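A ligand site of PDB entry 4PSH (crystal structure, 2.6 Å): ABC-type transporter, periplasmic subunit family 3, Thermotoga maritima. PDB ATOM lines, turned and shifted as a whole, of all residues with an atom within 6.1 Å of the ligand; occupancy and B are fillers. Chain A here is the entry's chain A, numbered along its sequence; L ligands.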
ATOM      1  N   LEU A  15     -14.077   6.393  17.744  1.00  0.00           N
ATOM      2  CA  LEU A  15     -15.435   6.220  17.191  1.00  0.00           C
ATOM      3  C   LEU A  15     -15.866   4.690  17.180  1.00  0.00           C
ATOM      4  O   LEU A  15     -15.055   3.788  17.412  1.00  0.00           O
ATOM      5  CB  LEU A  15     -15.543   6.877  15.799  1.00  0.00           C
ATOM      6  CG  LEU A  15     -14.468   6.471  14.757  1.00  0.00           C
ATOM      7  CD1 LEU A  15     -14.607   5.024  14.309  1.00  0.00           C
ATOM      8  CD2 LEU A  15     -14.428   7.396  13.516  1.00  0.00           C
ATOM      9  N   SER A  16     -17.154   4.433  16.940  1.00  0.00           N
ATOM     10  CA  SER A  16     -17.638   3.077  16.658  1.00  0.00           C
ATOM     11  C   SER A  16     -18.194   3.028  15.200  1.00  0.00           C
ATOM     12  O   SER A  16     -19.261   3.601  14.922  1.00  0.00           O
ATOM     13  CB  SER A  16     -18.724   2.706  17.651  1.00  0.00           C
ATOM     14  OG  SER A  16     -19.172   1.394  17.419  1.00  0.00           O
ATOM     15  N   ALA A  17     -17.453   2.378  14.312  1.00  0.00           N
ATOM     16  CA  ALA A  17     -17.746   2.345  12.896  1.00  0.00           C
ATOM     17  C   ALA A  17     -18.878   1.383  12.475  1.00  0.00           C
ATOM     18  O   ALA A  17     -18.731   0.594  11.542  1.00  0.00           O
ATOM     19  CB  ALA A  17     -16.466   2.105  12.088  1.00  0.00           C
ATOM     20  N   ASP A  18     -20.022   1.477  13.131  1.00  0.00           N
ATOM     21  CA  ASP A  18     -21.205   0.731  12.791  1.00  0.00           C
ATOM     22  C   ASP A  18     -22.356   1.709  12.683  1.00  0.00           C
ATOM     23  O   ASP A  18     -23.474   1.364  13.067  1.00  0.00           O
ATOM     24  CB  ASP A  18     -21.540  -0.271  13.913  1.00  0.00           C
ATOM     25  CG  ASP A  18     -21.648   0.404  15.325  1.00  0.00           C
ATOM     26  OD1 ASP A  18     -21.044   1.477  15.526  1.00  0.00           O
ATOM     27  OD2 ASP A  18     -22.317  -0.151  16.251  1.00  0.00           O
ATOM     28  N   PHE A  19     -22.095   2.911  12.174  1.00  0.00           N
ATOM     29  CA  PHE A  19     -23.094   3.996  12.190  1.00  0.00           C
ATOM     30  C   PHE A  19     -23.084   4.787  10.861  1.00  0.00           C
ATOM     31  O   PHE A  19     -22.773   5.996  10.858  1.00  0.00           O
ATOM     32  CB  PHE A  19     -22.775   4.923  13.361  1.00  0.00           C
ATOM     33  CG  PHE A  19     -23.971   5.704  13.931  1.00  0.00           C
ATOM     34  CD1 PHE A  19     -25.017   5.053  14.561  1.00  0.00           C
ATOM     35  CD2 PHE A  19     -23.961   7.102  13.939  1.00  0.00           C
ATOM     36  CE1 PHE A  19     -26.103   5.753  15.100  1.00  0.00           C
ATOM     37  CE2 PHE A  19     -25.030   7.824  14.502  1.00  0.00           C
ATOM     38  CZ  PHE A  19     -26.115   7.152  15.077  1.00  0.00           C
ATOM     39  N   GLU A  23     -19.801   6.917  10.472  1.00  0.00           N
ATOM     40  CA  GLU A  23     -18.599   6.119  10.558  1.00  0.00           C
ATOM     41  C   GLU A  23     -19.047   4.712  10.121  1.00  0.00           C
ATOM     42  O   GLU A  23     -20.043   4.185  10.671  1.00  0.00           O
ATOM     43  CB  GLU A  23     -18.197   5.894  12.013  1.00  0.00           C
ATOM     44  CG  GLU A  23     -17.957   7.043  12.883  1.00  0.00           C
ATOM     45  CD  GLU A  23     -19.194   7.769  13.410  1.00  0.00           C
ATOM     46  OE1 GLU A  23     -20.154   7.253  14.065  1.00  0.00           O
ATOM     47  OE2 GLU A  23     -19.138   8.964  13.145  1.00  0.00           O
ATOM     48  N   PHE A  57     -19.099   1.612  21.297  1.00  0.00           N
ATOM     49  CA  PHE A  57     -19.570   2.959  21.477  1.00  0.00           C
ATOM     50  C   PHE A  57     -19.614   3.392  22.988  1.00  0.00           C
ATOM     51  O   PHE A  57     -19.132   4.477  23.372  1.00  0.00           O
ATOM     52  CB  PHE A  57     -20.936   3.133  20.795  1.00  0.00           C
ATOM     53  CG  PHE A  57     -21.576   4.496  21.047  1.00  0.00           C
ATOM     54  CD1 PHE A  57     -21.255   5.582  20.262  1.00  0.00           C
ATOM     55  CD2 PHE A  57     -22.464   4.690  22.132  1.00  0.00           C
ATOM     56  CE1 PHE A  57     -21.792   6.811  20.522  1.00  0.00           C
ATOM     57  CE2 PHE A  57     -23.038   5.936  22.394  1.00  0.00           C
ATOM     58  CZ  PHE A  57     -22.697   7.000  21.583  1.00  0.00           C
ATOM     59  N   LEU A  60     -16.451   4.810  24.673  1.00  0.00           N
ATOM     60  CA  LEU A  60     -15.796   5.985  24.099  1.00  0.00           C
ATOM     61  C   LEU A  60     -15.488   7.020  25.187  1.00  0.00           C
ATOM     62  O   LEU A  60     -14.342   7.434  25.345  1.00  0.00           O
ATOM     63  CB  LEU A  60     -16.651   6.586  22.972  1.00  0.00           C
ATOM     64  CG  LEU A  60     -16.595   5.804  21.656  1.00  0.00           C
ATOM     65  CD1 LEU A  60     -17.658   6.210  20.672  1.00  0.00           C
ATOM     66  CD2 LEU A  60     -15.231   6.004  21.033  1.00  0.00           C
ATOM     67  N   SER A  74     -18.255  10.462  16.802  1.00  0.00           N
ATOM     68  CA  SER A  74     -18.909   9.209  16.610  1.00  0.00           C
ATOM     69  C   SER A  74     -20.409   9.318  16.671  1.00  0.00           C
ATOM     70  O   SER A  74     -21.033   8.605  17.375  1.00  0.00           O
ATOM     71  CB  SER A  74     -18.375   8.208  17.644  1.00  0.00           C
ATOM     72  OG  SER A  74     -18.825   6.913  17.426  1.00  0.00           O
ATOM     73  N   GLY A  75     -20.989  10.215  15.927  1.00  0.00           N
ATOM     74  CA  GLY A  75     -22.391  10.512  16.022  1.00  0.00           C
ATOM     75  C   GLY A  75     -22.969  10.612  17.408  1.00  0.00           C
ATOM     76  O   GLY A  75     -24.028  10.139  17.659  1.00  0.00           O
ATOM     77  N   MET A  76     -22.263  11.267  18.310  1.00  0.00           N
ATOM     78  CA  MET A  76     -22.633  11.328  19.699  1.00  0.00           C
ATOM     79  C   MET A  76     -23.582  12.459  19.980  1.00  0.00           C
ATOM     80  O   MET A  76     -23.304  13.575  19.734  1.00  0.00           O
ATOM     81  CB  MET A  76     -21.392  11.420  20.576  1.00  0.00           C
ATOM     82  CG  MET A  76     -21.607  11.260  22.098  1.00  0.00           C
ATOM     83  SD  MET A  76     -20.231  11.358  23.171  1.00  0.00           S
ATOM     84  CE  MET A  76     -19.911   9.743  23.253  1.00  0.00           C
ATOM     85  N   THR A  77     -24.727  12.120  20.504  1.00  0.00           N
ATOM     86  CA  THR A  77     -25.753  13.119  20.912  1.00  0.00           C
ATOM     87  C   THR A  77     -25.283  13.903  22.133  1.00  0.00           C
ATOM     88  O   THR A  77     -24.869  13.288  23.102  1.00  0.00           O
ATOM     89  CB  THR A  77     -27.080  12.440  21.349  1.00  0.00           C
ATOM     90  OG1 THR A  77     -27.584  11.567  20.342  1.00  0.00           O
ATOM     91  CG2 THR A  77     -28.158  13.461  21.687  1.00  0.00           C
ATOM     92  N   ILE A  78     -25.386  15.223  22.109  1.00  0.00           N
ATOM     93  CA  ILE A  78     -25.155  16.058  23.308  1.00  0.00           C
ATOM     94  C   ILE A  78     -26.262  15.887  24.343  1.00  0.00           C
ATOM     95  O   ILE A  78     -27.446  16.099  24.042  1.00  0.00           O
ATOM     96  CB  ILE A  78     -25.061  17.564  22.932  1.00  0.00           C
ATOM     97  CG1 ILE A  78     -23.902  17.782  21.984  1.00  0.00           C
ATOM     98  CG2 ILE A  78     -24.893  18.416  24.144  1.00  0.00           C
ATOM     99  CD1 ILE A  78     -24.102  18.977  21.016  1.00  0.00           C
ATOM    100  N   ARG A  82     -24.296  13.417  29.789  1.00  0.00           N
ATOM    101  CA  ARG A  82     -22.892  13.328  29.317  1.00  0.00           C
ATOM    102  C   ARG A  82     -22.105  14.583  29.662  1.00  0.00           C
ATOM    103  O   ARG A  82     -20.906  14.500  29.927  1.00  0.00           O
ATOM    104  CB  ARG A  82     -22.772  12.991  27.841  1.00  0.00           C
ATOM    105  CG  ARG A  82     -23.165  11.525  27.538  1.00  0.00           C
ATOM    106  CD  ARG A  82     -23.706  11.393  26.114  1.00  0.00           C
ATOM    107  NE  ARG A  82     -24.083  10.032  25.796  1.00  0.00           N
ATOM    108  CZ  ARG A  82     -24.622   9.640  24.633  1.00  0.00           C
ATOM    109  NH1 ARG A  82     -24.846  10.553  23.643  1.00  0.00           N
ATOM    110  NH2 ARG A  82     -24.952   8.342  24.444  1.00  0.00           N
ATOM    111  N   GLN A  97     -34.742   9.501  17.531  1.00  0.00           N
ATOM    112  CA  GLN A  97     -34.902   8.050  17.472  1.00  0.00           C
ATOM    113  C   GLN A  97     -36.050   7.634  16.558  1.00  0.00           C
ATOM    114  O   GLN A  97     -37.072   8.332  16.462  1.00  0.00           O
ATOM    115  CB  GLN A  97     -35.067   7.438  18.853  1.00  0.00           C
ATOM    116  CG  GLN A  97     -33.940   7.751  19.881  1.00  0.00           C
ATOM    117  CD  GLN A  97     -32.537   7.378  19.404  1.00  0.00           C
ATOM    118  OE1 GLN A  97     -31.656   8.258  19.297  1.00  0.00           O
ATOM    119  NE2 GLN A  97     -32.304   6.087  19.096  1.00  0.00           N
ATOM    120  N   GLN A 123     -28.272  -0.528  20.835  1.00  0.00           N
ATOM    121  CA  GLN A 123     -26.848  -0.439  21.179  1.00  0.00           C
ATOM    122  C   GLN A 123     -26.703   0.134  22.591  1.00  0.00           C
ATOM    123  O   GLN A 123     -27.323   1.199  22.926  1.00  0.00           O
ATOM    124  CB  GLN A 123     -26.085   0.406  20.184  1.00  0.00           C
ATOM    125  CG  GLN A 123     -24.679   0.752  20.615  1.00  0.00           C
ATOM    126  CD  GLN A 123     -23.889   1.257  19.446  1.00  0.00           C
ATOM    127  OE1 GLN A 123     -24.007   2.432  19.058  1.00  0.00           O
ATOM    128  NE2 GLN A 123     -23.079   0.368  18.850  1.00  0.00           N
ATOM    129  N   GLY A 125     -25.669   1.919  25.823  1.00  0.00           N
ATOM    130  CA  GLY A 125     -25.195   3.251  26.117  1.00  0.00           C
ATOM    131  C   GLY A 125     -25.742   4.317  25.198  1.00  0.00           C
ATOM    132  O   GLY A 125     -25.477   5.481  25.451  1.00  0.00           O
ATOM    133  N   THR A 126     -26.480   3.958  24.146  1.00  0.00           N
ATOM    134  CA  THR A 126     -27.005   4.981  23.279  1.00  0.00           C
ATOM    135  C   THR A 126     -28.252   5.652  23.874  1.00  0.00           C
ATOM    136  O   THR A 126     -28.815   5.156  24.873  1.00  0.00           O
ATOM    137  CB  THR A 126     -27.343   4.468  21.901  1.00  0.00           C
ATOM    138  OG1 THR A 126     -28.402   3.520  22.040  1.00  0.00           O
ATOM    139  CG2 THR A 126     -26.115   3.865  21.207  1.00  0.00           C
ATOM    140  N   THR A 127     -28.698   6.767  23.270  1.00  0.00           N
ATOM    141  CA  THR A 127     -29.943   7.422  23.686  1.00  0.00           C
ATOM    142  C   THR A 127     -31.153   6.538  23.337  1.00  0.00           C
ATOM    143  O   THR A 127     -32.206   6.591  23.988  1.00  0.00           O
ATOM    144  CB  THR A 127     -30.061   8.867  23.059  1.00  0.00           C
ATOM    145  OG1 THR A 127     -29.633   8.838  21.700  1.00  0.00           O
ATOM    146  CG2 THR A 127     -29.160   9.874  23.751  1.00  0.00           C
ATOM    147  N   GLY A 128     -31.009   5.684  22.321  1.00  0.00           N
ATOM    148  CA  GLY A 128     -32.004   4.625  22.064  1.00  0.00           C
ATOM    149  C   GLY A 128     -32.168   3.777  23.300  1.00  0.00           C
ATOM    150  O   GLY A 128     -33.267   3.622  23.823  1.00  0.00           O
ATOM    151  N   PHE A 146     -24.178  -2.175  16.449  1.00  0.00           N
ATOM    152  CA  PHE A 146     -25.497  -2.175  15.752  1.00  0.00           C
ATOM    153  C   PHE A 146     -25.590  -3.309  14.737  1.00  0.00           C
ATOM    154  O   PHE A 146     -26.672  -3.749  14.366  1.00  0.00           O
ATOM    155  CB  PHE A 146     -25.780  -0.845  15.042  1.00  0.00           C
ATOM    156  CG  PHE A 146     -26.429   0.192  15.914  1.00  0.00           C
ATOM    157  CD1 PHE A 146     -27.671  -0.063  16.536  1.00  0.00           C
ATOM    158  CD2 PHE A 146     -25.824   1.428  16.100  1.00  0.00           C
ATOM    159  CE1 PHE A 146     -28.282   0.911  17.368  1.00  0.00           C
ATOM    160  CE2 PHE A 146     -26.426   2.408  16.919  1.00  0.00           C
ATOM    161  CZ  PHE A 146     -27.658   2.152  17.563  1.00  0.00           C
ATOM    162  N   ASP A 164     -31.051   6.036  15.916  1.00  0.00           N
ATOM    163  CA  ASP A 164     -31.144   7.336  15.293  1.00  0.00           C
ATOM    164  C   ASP A 164     -31.631   7.222  13.835  1.00  0.00           C
ATOM    165  O   ASP A 164     -31.144   6.397  13.071  1.00  0.00           O
ATOM    166  CB  ASP A 164     -29.795   8.025  15.295  1.00  0.00           C
ATOM    167  CG  ASP A 164     -29.245   8.245  16.667  1.00  0.00           C
ATOM    168  OD1 ASP A 164     -29.379   7.360  17.555  1.00  0.00           O
ATOM    169  OD2 ASP A 164     -28.606   9.308  16.843  1.00  0.00           O
ATOM    170  N   GLU A 188     -32.421  15.491  18.867  1.00  0.00           N
ATOM    171  CA  GLU A 188     -31.065  15.251  19.360  1.00  0.00           C
ATOM    172  C   GLU A 188     -30.115  15.979  18.463  1.00  0.00           C
ATOM    173  O   GLU A 188     -30.419  16.180  17.262  1.00  0.00           O
ATOM    174  CB  GLU A 188     -30.747  13.742  19.382  1.00  0.00           C
ATOM    175  CG  GLU A 188     -31.705  12.967  20.297  1.00  0.00           C
ATOM    176  CD  GLU A 188     -31.370  11.493  20.451  1.00  0.00           C
ATOM    177  OE1 GLU A 188     -30.133  11.112  20.366  1.00  0.00           O
ATOM    178  OE2 GLU A 188     -32.371  10.725  20.676  1.00  0.00           O
ATOM    179  N   TYR A 190     -25.828  16.110  17.408  1.00  0.00           N
ATOM    180  CA  TYR A 190     -24.501  15.509  17.554  1.00  0.00           C
ATOM    181  C   TYR A 190     -23.478  16.575  17.915  1.00  0.00           C
ATOM    182  O   TYR A 190     -23.547  17.701  17.424  1.00  0.00           O
ATOM    183  CB  TYR A 190     -24.070  14.760  16.273  1.00  0.00           C
ATOM    184  CG  TYR A 190     -24.997  13.630  15.886  1.00  0.00           C
ATOM    185  CD1 TYR A 190     -25.990  13.187  16.753  1.00  0.00           C
ATOM    186  CD2 TYR A 190     -24.850  12.981  14.658  1.00  0.00           C
ATOM    187  CE1 TYR A 190     -26.865  12.153  16.399  1.00  0.00           C
ATOM    188  CE2 TYR A 190     -25.681  11.925  14.280  1.00  0.00           C
ATOM    189  CZ  TYR A 190     -26.711  11.517  15.151  1.00  0.00           C
ATOM    190  OH  TYR A 190     -27.568  10.478  14.784  1.00  0.00           O
HETATM  191  N1  LIG L   1     -26.678   9.210  18.906  1.00  0.00           N
HETATM  192  C1  LIG L   1     -26.644   8.044  19.790  1.00  0.00           C
HETATM  193  C2  LIG L   1     -25.909   8.394  21.055  1.00  0.00           C
HETATM  194  O1  LIG L   1     -25.226   9.424  21.171  1.00  0.00           O
HETATM  195  C3  LIG L   1     -25.890   6.844  19.189  1.00  0.00           C
HETATM  196  C4  LIG L   1     -25.117   7.139  17.959  1.00  0.00           C
HETATM  197  C5  LIG L   1     -23.637   6.804  17.922  1.00  0.00           C
HETATM  198  N2  LIG L   1     -23.309   5.417  17.658  1.00  0.00           N
HETATM  199  C6  LIG L   1     -22.244   4.960  16.977  1.00  0.00           C
HETATM  200  N3  LIG L   1     -21.361   5.768  16.396  1.00  0.00           N
HETATM  201  N4  LIG L   1     -22.071   3.638  16.873  1.00  0.00           N
HETATM  202  O2  LIG L   1     -25.997   7.609  21.997  1.00  0.00           O
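The backbone carbonyl oxygen of Ser 74 lies within hydrogen-bond range of a nitrogen (N3) of the ligand, 3.0 Å away. N1 of the ligand lies within hydrogen-bond range of OG1 of Thr 77. OD2 of Asp 164 lies within salt-bridge range of N1 of the ligand, 2.8 Å away. A nitrogen (N3) of the ligand lies within hydrogen-bond range of the backbone carbonyl oxygen (O) of Ser 16 (3.4 Å). An oxygen (O1) of the ligand lies within hydrogen-bond range of the backbone NH (N) of Thr 77, at 2.8 Å. N3 of the ligand lies within salt-bridge range of OE1 of Glu 23 (3.0 Å). An oxygen (O1) of the ligand lies within salt-bridge range of the guanidinium group (NH1) of Arg 82 (2.7 Å). The side-chain carboxylate of Asp 18 is in salt-bridge range of a nitrogen (N4) of the ligand. The backbone carbonyl oxygen of Gly 75 lies within hydrogen-bond range of a nitrogen (N1) of the ligand, 3.1 Å away. An oxygen (O2) of the ligand sits at hydrogen-bond distance from the backbone NH (N) of Thr 127 (3.1 Å). OG of Ser 74 is in hydrogen-bond range of N3 of the ligand (3.0 Å). The side-chain amide oxygen of Gln 123 sits at hydrogen-bond distance from a nitrogen (N4) of the ligand, at 3.2 Å.
OD1 of Asp 164 lies close to OE1 of Gln 97 (3.0 Å). The side-chain carboxylate (OD2) of Asp 18 lies within hydrogen-bond range of the backbone NH (N) of Phe 146 (2.8 Å). The side-chain carboxylate (OD2) of Asp 18 lies within hydrogen-bond range of the side-chain amide nitrogen (NE2) of Gln 123, at 2.8 Å. OE1 of Gln 97 is in hydrogen-bond range of OG1 of Thr 127, 3.2 Å away. N of Gly 128 sits close to OG1 of Thr 126 (3.4 Å). The side-chain carboxylate (OE1) of Glu 188 is in hydrogen-bond range of the side-chain hydroxyl (OG1) of Thr 77 (2.6 Å). The side-chain hydroxyl of Ser 74 lies within hydrogen-bond range of the backbone NH of Ser 16 (3.0 Å). OE1 of Glu 188 sits at hydrogen-bond distance from OG1 of Thr 127 (2.7 Å).
Phe 19 touches the ligand. CE1 of Phe 57 touches C5 of the ligand, 3.2 Å away. Met 76 touches the ligand. Thr 126 touches the ligand (CA to O2, 3.1 Å). CE1 of Tyr 190 touches N1 of the ligand, 3.9 Å away. Within 4 Å of the ligand: Ser 16, Asp 18, Phe 19, Glu 23, Phe 57, Ser 74, Gly 75, Met 76, Thr 77, Arg 82, Gln 123, Thr 126, Thr 127, Asp 164 and Tyr 190.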
